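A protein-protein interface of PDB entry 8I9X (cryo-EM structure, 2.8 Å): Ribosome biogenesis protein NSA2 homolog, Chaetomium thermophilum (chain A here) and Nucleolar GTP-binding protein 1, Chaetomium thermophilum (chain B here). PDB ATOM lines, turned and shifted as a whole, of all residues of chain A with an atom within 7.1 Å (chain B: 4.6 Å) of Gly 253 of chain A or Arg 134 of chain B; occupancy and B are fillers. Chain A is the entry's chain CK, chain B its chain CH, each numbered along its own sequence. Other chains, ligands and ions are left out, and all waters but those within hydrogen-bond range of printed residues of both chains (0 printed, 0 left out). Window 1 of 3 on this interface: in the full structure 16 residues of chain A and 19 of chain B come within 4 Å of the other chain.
OH of Tyr 111 of chain B is in hydrogen-bond range of N of Gly 253 of chain A (3.1 Å).
The side-chain hydroxyl (OH) of Tyr 179 of chain A sits close to the backbone carbonyl oxygen (O) of Gly 253 of chain A (3.2 Å). The backbone carbonyl oxygen (O) of Cys 254 of chain A lies within hydrogen-bond range of the side-chain amide nitrogen (ND2) of Asn 247 of chain A.
Arg 134 of chain B touches two residues of chain A. No residue of chain A comes within 4 Å of Gly 133 of chain B. Printed residues of chain A within 4 Å of Leu 114 of chain B: Tyr 179 and Gly 253. Of the printed residues of chain B, Cys 254 of chain A touches Arg 134 (3.97 Å). Of the printed residues of chain B, Tyr 179 of chain A touches Leu 114. Of the printed residues of chain A, Tyr 111 of chain B touches Gly 253 (3.1 Å). Asn 248 of chain A touches none of the printed residues of chain B. Ala 136 of chain B touches none of the printed residues of chain A. The nearest residue of chain B that does not touch Gly 253 of chain A is Ala 130 of chain B (4.5 Å). The nearest residue of chain A that does not touch Arg 134 of chain B is Asn 183 of chain A (6.3 Å). The nearest printed residue of chain B that does not touch Tyr 179 of chain A is Tyr 111 of chain B (6.0 Å).
Of the 12 printed residues of chain B, 3 touch a printed residue of chain A. Hydrophobic or aromatic side chains of chain B within 4 Å of the printed part of chain A: Tyr 111 and Leu 114. Of the 11 printed residues of chain A, 3 touch a printed residue of chain B. Among the printed residues, 5 pairs touch across the chains.
Tyr 179 of chain A touches Leu 114 of chain B (OH to CD1, 3.6 Å). CD1 of Leu 114 of chain B touches CA of Gly 253 of chain A, 3.7 Å away. Gly 253 of chain A touches Arg 134 of chain B (O to NH1, 3.8 Å). Cys 254 of chain A touches Arg 134 of chain B.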
ATOM      1  N   TYR A 179      -7.205 -11.079  17.714  1.00  0.00           N
ATOM      2  CA  TYR A 179      -6.829 -10.078  18.703  1.00  0.00           C
ATOM      3  C   TYR A 179      -8.089  -9.443  19.275  1.00  0.00           C
ATOM      4  O   TYR A 179      -9.079  -9.265  18.561  1.00  0.00           O
ATOM      5  CB  TYR A 179      -5.930  -8.988  18.097  1.00  0.00           C
ATOM      6  CG  TYR A 179      -4.464  -9.357  18.063  1.00  0.00           C
ATOM      7  CD1 TYR A 179      -3.911  -9.968  16.949  1.00  0.00           C
ATOM      8  CD2 TYR A 179      -3.639  -9.106  19.148  1.00  0.00           C
ATOM      9  CE1 TYR A 179      -2.578 -10.315  16.913  1.00  0.00           C
ATOM     10  CE2 TYR A 179      -2.303  -9.449  19.120  1.00  0.00           C
ATOM     11  CZ  TYR A 179      -1.779 -10.053  17.999  1.00  0.00           C
ATOM     12  OH  TYR A 179      -0.451 -10.401  17.959  1.00  0.00           O
ATOM     13  N   ASN A 183      -3.564  -1.235  21.948  1.00  0.00           N
ATOM     14  CA  ASN A 183      -2.933  -0.116  22.640  1.00  0.00           C
ATOM     15  C   ASN A 183      -3.351   1.150  21.908  1.00  0.00           C
ATOM     16  O   ASN A 183      -2.865   1.439  20.812  1.00  0.00           O
ATOM     17  CB  ASN A 183      -1.418  -0.280  22.666  1.00  0.00           C
ATOM     18  CG  ASN A 183      -0.993  -1.651  23.139  1.00  0.00           C
ATOM     19  OD1 ASN A 183      -1.263  -2.038  24.275  1.00  0.00           O
ATOM     20  ND2 ASN A 183      -0.322  -2.393  22.270  1.00  0.00           N
ATOM     21  N   ASN A 247       0.069   0.612  12.949  1.00  0.00           N
ATOM     22  CA  ASN A 247       1.233  -0.261  12.912  1.00  0.00           C
ATOM     23  C   ASN A 247       0.939  -1.421  11.970  1.00  0.00           C
ATOM     24  O   ASN A 247      -0.113  -1.477  11.329  1.00  0.00           O
ATOM     25  CB  ASN A 247       1.603  -0.760  14.314  1.00  0.00           C
ATOM     26  CG  ASN A 247       0.678  -1.852  14.808  1.00  0.00           C
ATOM     27  OD1 ASN A 247      -0.541  -1.751  14.689  1.00  0.00           O
ATOM     28  ND2 ASN A 247       1.256  -2.904  15.372  1.00  0.00           N
ATOM     29  N   ASN A 248       1.886  -2.353  11.879  1.00  0.00           N
ATOM     30  CA  ASN A 248       1.734  -3.559  11.069  1.00  0.00           C
ATOM     31  C   ASN A 248       1.520  -4.738  12.004  1.00  0.00           C
ATOM     32  O   ASN A 248       2.489  -5.385  12.426  1.00  0.00           O
ATOM     33  CB  ASN A 248       2.963  -3.784  10.183  1.00  0.00           C
ATOM     34  CG  ASN A 248       2.860  -3.067   8.853  1.00  0.00           C
ATOM     35  OD1 ASN A 248       3.474  -2.023   8.648  1.00  0.00           O
ATOM     36  ND2 ASN A 248       2.077  -3.626   7.942  1.00  0.00           N
ATOM     37  N   PRO A 249       0.276  -5.059  12.362  1.00  0.00           N
ATOM     38  CA  PRO A 249       0.036  -6.134  13.334  1.00  0.00           C
ATOM     39  C   PRO A 249       0.497  -7.497  12.846  1.00  0.00           C
ATOM     40  O   PRO A 249       0.686  -8.417  13.647  1.00  0.00           O
ATOM     41  CB  PRO A 249      -1.486  -6.092  13.528  1.00  0.00           C
ATOM     42  CG  PRO A 249      -1.880  -4.716  13.105  1.00  0.00           C
ATOM     43  CD  PRO A 249      -0.979  -4.413  11.955  1.00  0.00           C
ATOM     44  N   GLU A 250       0.669  -7.648  11.535  1.00  0.00           N
ATOM     45  CA  GLU A 250       1.172  -8.901  10.991  1.00  0.00           C
ATOM     46  C   GLU A 250       2.658  -9.092  11.278  1.00  0.00           C
ATOM     47  O   GLU A 250       3.131 -10.231  11.347  1.00  0.00           O
ATOM     48  CB  GLU A 250       0.906  -8.967   9.485  1.00  0.00           C
ATOM     49  CG  GLU A 250       1.707  -7.982   8.653  1.00  0.00           C
ATOM     50  CD  GLU A 250       1.033  -6.630   8.532  1.00  0.00           C
ATOM     51  OE1 GLU A 250       0.112  -6.345   9.327  1.00  0.00           O
ATOM     52  OE2 GLU A 250       1.423  -5.851   7.637  1.00  0.00           O
ATOM     53  N   ASN A 251       3.400  -8.000  11.452  1.00  0.00           N
ATOM     54  CA  ASN A 251       4.823  -8.065  11.763  1.00  0.00           C
ATOM     55  C   ASN A 251       5.086  -7.863  13.252  1.00  0.00           C
ATOM     56  O   ASN A 251       6.103  -8.325  13.775  1.00  0.00           O
ATOM     57  CB  ASN A 251       5.588  -7.021  10.947  1.00  0.00           C
ATOM     58  CG  ASN A 251       5.331  -7.141   9.463  1.00  0.00           C
ATOM     59  OD1 ASN A 251       4.664  -6.297   8.868  1.00  0.00           O
ATOM     60  ND2 ASN A 251       5.852  -8.199   8.855  1.00  0.00           N
ATOM     61  N   ASP A 252       4.187  -7.167  13.937  1.00  0.00           N
ATOM     62  CA  ASP A 252       4.306  -6.904  15.363  1.00  0.00           C
ATOM     63  C   ASP A 252       3.174  -7.610  16.095  1.00  0.00           C
ATOM     64  O   ASP A 252       2.001  -7.409  15.768  1.00  0.00           O
ATOM     65  CB  ASP A 252       4.251  -5.403  15.640  1.00  0.00           C
ATOM     66  CG  ASP A 252       5.219  -4.619  14.785  1.00  0.00           C
ATOM     67  OD1 ASP A 252       6.334  -5.121  14.530  1.00  0.00           O
ATOM     68  OD2 ASP A 252       4.859  -3.504  14.354  1.00  0.00           O
ATOM     69  N   GLY A 253       3.520  -8.414  17.094  1.00  0.00           N
ATOM     70  CA  GLY A 253       2.505  -9.163  17.810  1.00  0.00           C
ATOM     71  C   GLY A 253       1.678  -8.312  18.752  1.00  0.00           C
ATOM     72  O   GLY A 253       1.453  -8.688  19.906  1.00  0.00           O
ATOM     73  N   CYS A 254       1.216  -7.165  18.264  1.00  0.00           N
ATOM     74  CA  CYS A 254       0.394  -6.239  19.030  1.00  0.00           C
ATOM     75  C   CYS A 254      -0.313  -5.316  18.051  1.00  0.00           C
ATOM     76  O   CYS A 254       0.136  -5.125  16.917  1.00  0.00           O
ATOM     77  CB  CYS A 254       1.225  -5.427  20.026  1.00  0.00           C
ATOM     78  SG  CYS A 254       2.368  -4.258  19.260  1.00  0.00           S
ATOM     79  N   VAL A 255      -1.424  -4.744  18.503  1.00  0.00           N
ATOM     80  CA  VAL A 255      -2.242  -3.845  17.699  1.00  0.00           C
ATOM     81  C   VAL A 255      -2.137  -2.454  18.310  1.00  0.00           C
ATOM     82  O   VAL A 255      -2.419  -2.269  19.499  1.00  0.00           O
ATOM     83  CB  VAL A 255      -3.701  -4.320  17.636  1.00  0.00           C
ATOM     84  CG1 VAL A 255      -4.553  -3.308  16.915  1.00  0.00           C
ATOM     85  CG2 VAL A 255      -3.788  -5.670  16.949  1.00  0.00           C
ATOM     86  N   ILE B 107       4.518 -14.470  26.167  1.00  0.00           N
ATOM     87  CA  ILE B 107       5.054 -13.871  24.950  1.00  0.00           C
ATOM     88  C   ILE B 107       5.550 -14.953  24.006  1.00  0.00           C
ATOM     89  O   ILE B 107       5.289 -14.913  22.794  1.00  0.00           O
ATOM     90  CB  ILE B 107       6.176 -12.872  25.291  1.00  0.00           C
ATOM     91  CG1 ILE B 107       5.607 -11.627  25.967  1.00  0.00           C
ATOM     92  CG2 ILE B 107       6.945 -12.487  24.040  1.00  0.00           C
ATOM     93  CD1 ILE B 107       6.669 -10.725  26.556  1.00  0.00           C
ATOM     94  N   TYR B 111       4.000 -15.639  20.241  1.00  0.00           N
ATOM     95  CA  TYR B 111       4.804 -15.461  19.041  1.00  0.00           C
ATOM     96  C   TYR B 111       5.101 -16.783  18.347  1.00  0.00           C
ATOM     97  O   TYR B 111       5.339 -16.792  17.137  1.00  0.00           O
ATOM     98  CB  TYR B 111       6.086 -14.706  19.375  1.00  0.00           C
ATOM     99  CG  TYR B 111       5.861 -13.217  19.453  1.00  0.00           C
ATOM    100  CD1 TYR B 111       5.547 -12.603  20.655  1.00  0.00           C
ATOM    101  CD2 TYR B 111       5.933 -12.429  18.316  1.00  0.00           C
ATOM    102  CE1 TYR B 111       5.331 -11.243  20.723  1.00  0.00           C
ATOM    103  CE2 TYR B 111       5.718 -11.073  18.376  1.00  0.00           C
ATOM    104  CZ  TYR B 111       5.418 -10.484  19.582  1.00  0.00           C
ATOM    105  OH  TYR B 111       5.203  -9.129  19.639  1.00  0.00           O
ATOM    106  N   LEU B 114       2.135 -17.055  16.187  1.00  0.00           N
ATOM    107  CA  LEU B 114       2.277 -16.100  15.091  1.00  0.00           C
ATOM    108  C   LEU B 114       3.257 -16.605  14.034  1.00  0.00           C
ATOM    109  O   LEU B 114       3.000 -16.481  12.830  1.00  0.00           O
ATOM    110  CB  LEU B 114       2.707 -14.740  15.634  1.00  0.00           C
ATOM    111  CG  LEU B 114       1.614 -14.007  16.409  1.00  0.00           C
ATOM    112  CD1 LEU B 114       2.162 -12.755  17.064  1.00  0.00           C
ATOM    113  CD2 LEU B 114       0.450 -13.673  15.496  1.00  0.00           C
ATOM    114  N   ALA B 130      10.405  -8.867  17.459  1.00  0.00           N
ATOM    115  CA  ALA B 130       9.405  -8.344  18.380  1.00  0.00           C
ATOM    116  C   ALA B 130       9.406  -9.121  19.689  1.00  0.00           C
ATOM    117  O   ALA B 130       9.392  -8.532  20.778  1.00  0.00           O
ATOM    118  CB  ALA B 130       8.025  -8.380  17.725  1.00  0.00           C
ATOM    119  N   ALA B 131       9.432 -10.453  19.601  1.00  0.00           N
ATOM    120  CA  ALA B 131       9.420 -11.267  20.814  1.00  0.00           C
ATOM    121  C   ALA B 131      10.652 -10.998  21.672  1.00  0.00           C
ATOM    122  O   ALA B 131      10.553 -10.806  22.896  1.00  0.00           O
ATOM    123  CB  ALA B 131       9.326 -12.747  20.446  1.00  0.00           C
ATOM    124  N   LEU B 132      11.826 -10.967  21.040  1.00  0.00           N
ATOM    125  CA  LEU B 132      13.055 -10.726  21.782  1.00  0.00           C
ATOM    126  C   LEU B 132      13.092  -9.335  22.406  1.00  0.00           C
ATOM    127  O   LEU B 132      13.509  -9.197  23.564  1.00  0.00           O
ATOM    128  CB  LEU B 132      14.261 -10.933  20.869  1.00  0.00           C
ATOM    129  CG  LEU B 132      14.879 -12.333  20.895  1.00  0.00           C
ATOM    130  CD1 LEU B 132      13.848 -13.406  20.588  1.00  0.00           C
ATOM    131  CD2 LEU B 132      16.030 -12.416  19.918  1.00  0.00           C
ATOM    132  N   GLY B 133      12.659  -8.307  21.671  1.00  0.00           N
ATOM    133  CA  GLY B 133      12.592  -6.974  22.235  1.00  0.00           C
ATOM    134  C   GLY B 133      11.629  -6.858  23.392  1.00  0.00           C
ATOM    135  O   GLY B 133      11.916  -6.155  24.366  1.00  0.00           O
ATOM    136  N   ARG B 134      10.485  -7.540  23.317  1.00  0.00           N
ATOM    137  CA  ARG B 134       9.570  -7.548  24.452  1.00  0.00           C
ATOM    138  C   ARG B 134      10.193  -8.193  25.682  1.00  0.00           C
ATOM    139  O   ARG B 134      10.071  -7.650  26.789  1.00  0.00           O
ATOM    140  CB  ARG B 134       8.275  -8.264  24.079  1.00  0.00           C
ATOM    141  CG  ARG B 134       7.443  -7.536  23.042  1.00  0.00           C
ATOM    142  CD  ARG B 134       6.312  -8.412  22.555  1.00  0.00           C
ATOM    143  NE  ARG B 134       5.279  -8.588  23.567  1.00  0.00           N
ATOM    144  CZ  ARG B 134       4.092  -8.002  23.532  1.00  0.00           C
ATOM    145  NH1 ARG B 134       3.739  -7.218  22.529  1.00  0.00           N
ATOM    146  NH2 ARG B 134       3.233  -8.215  24.526  1.00  0.00           N
ATOM    147  N   MET B 135      10.873  -9.329  25.514  1.00  0.00           N
ATOM    148  CA  MET B 135      11.540  -9.946  26.660  1.00  0.00           C
ATOM    149  C   MET B 135      12.587  -9.010  27.259  1.00  0.00           C
ATOM    150  O   MET B 135      12.683  -8.867  28.492  1.00  0.00           O
ATOM    151  CB  MET B 135      12.180 -11.269  26.242  1.00  0.00           C
ATOM    152  CG  MET B 135      11.187 -12.349  25.867  1.00  0.00           C
ATOM    153  SD  MET B 135      11.993 -13.894  25.413  1.00  0.00           S
ATOM    154  CE  MET B 135      10.783 -14.586  24.292  1.00  0.00           C
ATOM    155  N   ALA B 136      13.373  -8.357  26.401  1.00  0.00           N
ATOM    156  CA  ALA B 136      14.372  -7.411  26.884  1.00  0.00           C
ATOM    157  C   ALA B 136      13.720  -6.259  27.638  1.00  0.00           C
ATOM    158  O   ALA B 136      14.266  -5.765  28.632  1.00  0.00           O
ATOM    159  CB  ALA B 136      15.208  -6.891  25.715  1.00  0.00           C
ATOM    160  N   THR B 137      12.555  -5.808  27.171  1.00  0.00           N
ATOM    161  CA  THR B 137      11.844  -4.728  27.846  1.00  0.00           C
ATOM    162  C   THR B 137      11.385  -5.149  29.239  1.00  0.00           C
ATOM    163  O   THR B 137      11.501  -4.382  30.203  1.00  0.00           O
ATOM    164  CB  THR B 137      10.658  -4.274  26.995  1.00  0.00           C
ATOM    165  OG1 THR B 137      11.104  -4.018  25.659  1.00  0.00           O
ATOM    166  CG2 THR B 137      10.046  -3.007  27.567  1.00  0.00           C
ATOM    167  N   LEU B 138      10.866  -6.374  29.365  1.00  0.00           N
ATOM    168  CA  LEU B 138      10.491  -6.859  30.694  1.00  0.00           C
ATOM    169  C   LEU B 138      11.693  -6.923  31.631  1.00  0.00           C
ATOM    170  O   LEU B 138      11.588  -6.560  32.809  1.00  0.00           O
ATOM    171  CB  LEU B 138       9.799  -8.221  30.616  1.00  0.00           C
ATOM    172  CG  LEU B 138       8.303  -8.289  30.283  1.00  0.00           C
ATOM    173  CD1 LEU B 138       7.960  -7.951  28.852  1.00  0.00           C
ATOM    174  CD2 LEU B 138       7.783  -9.668  30.633  1.00  0.00           C
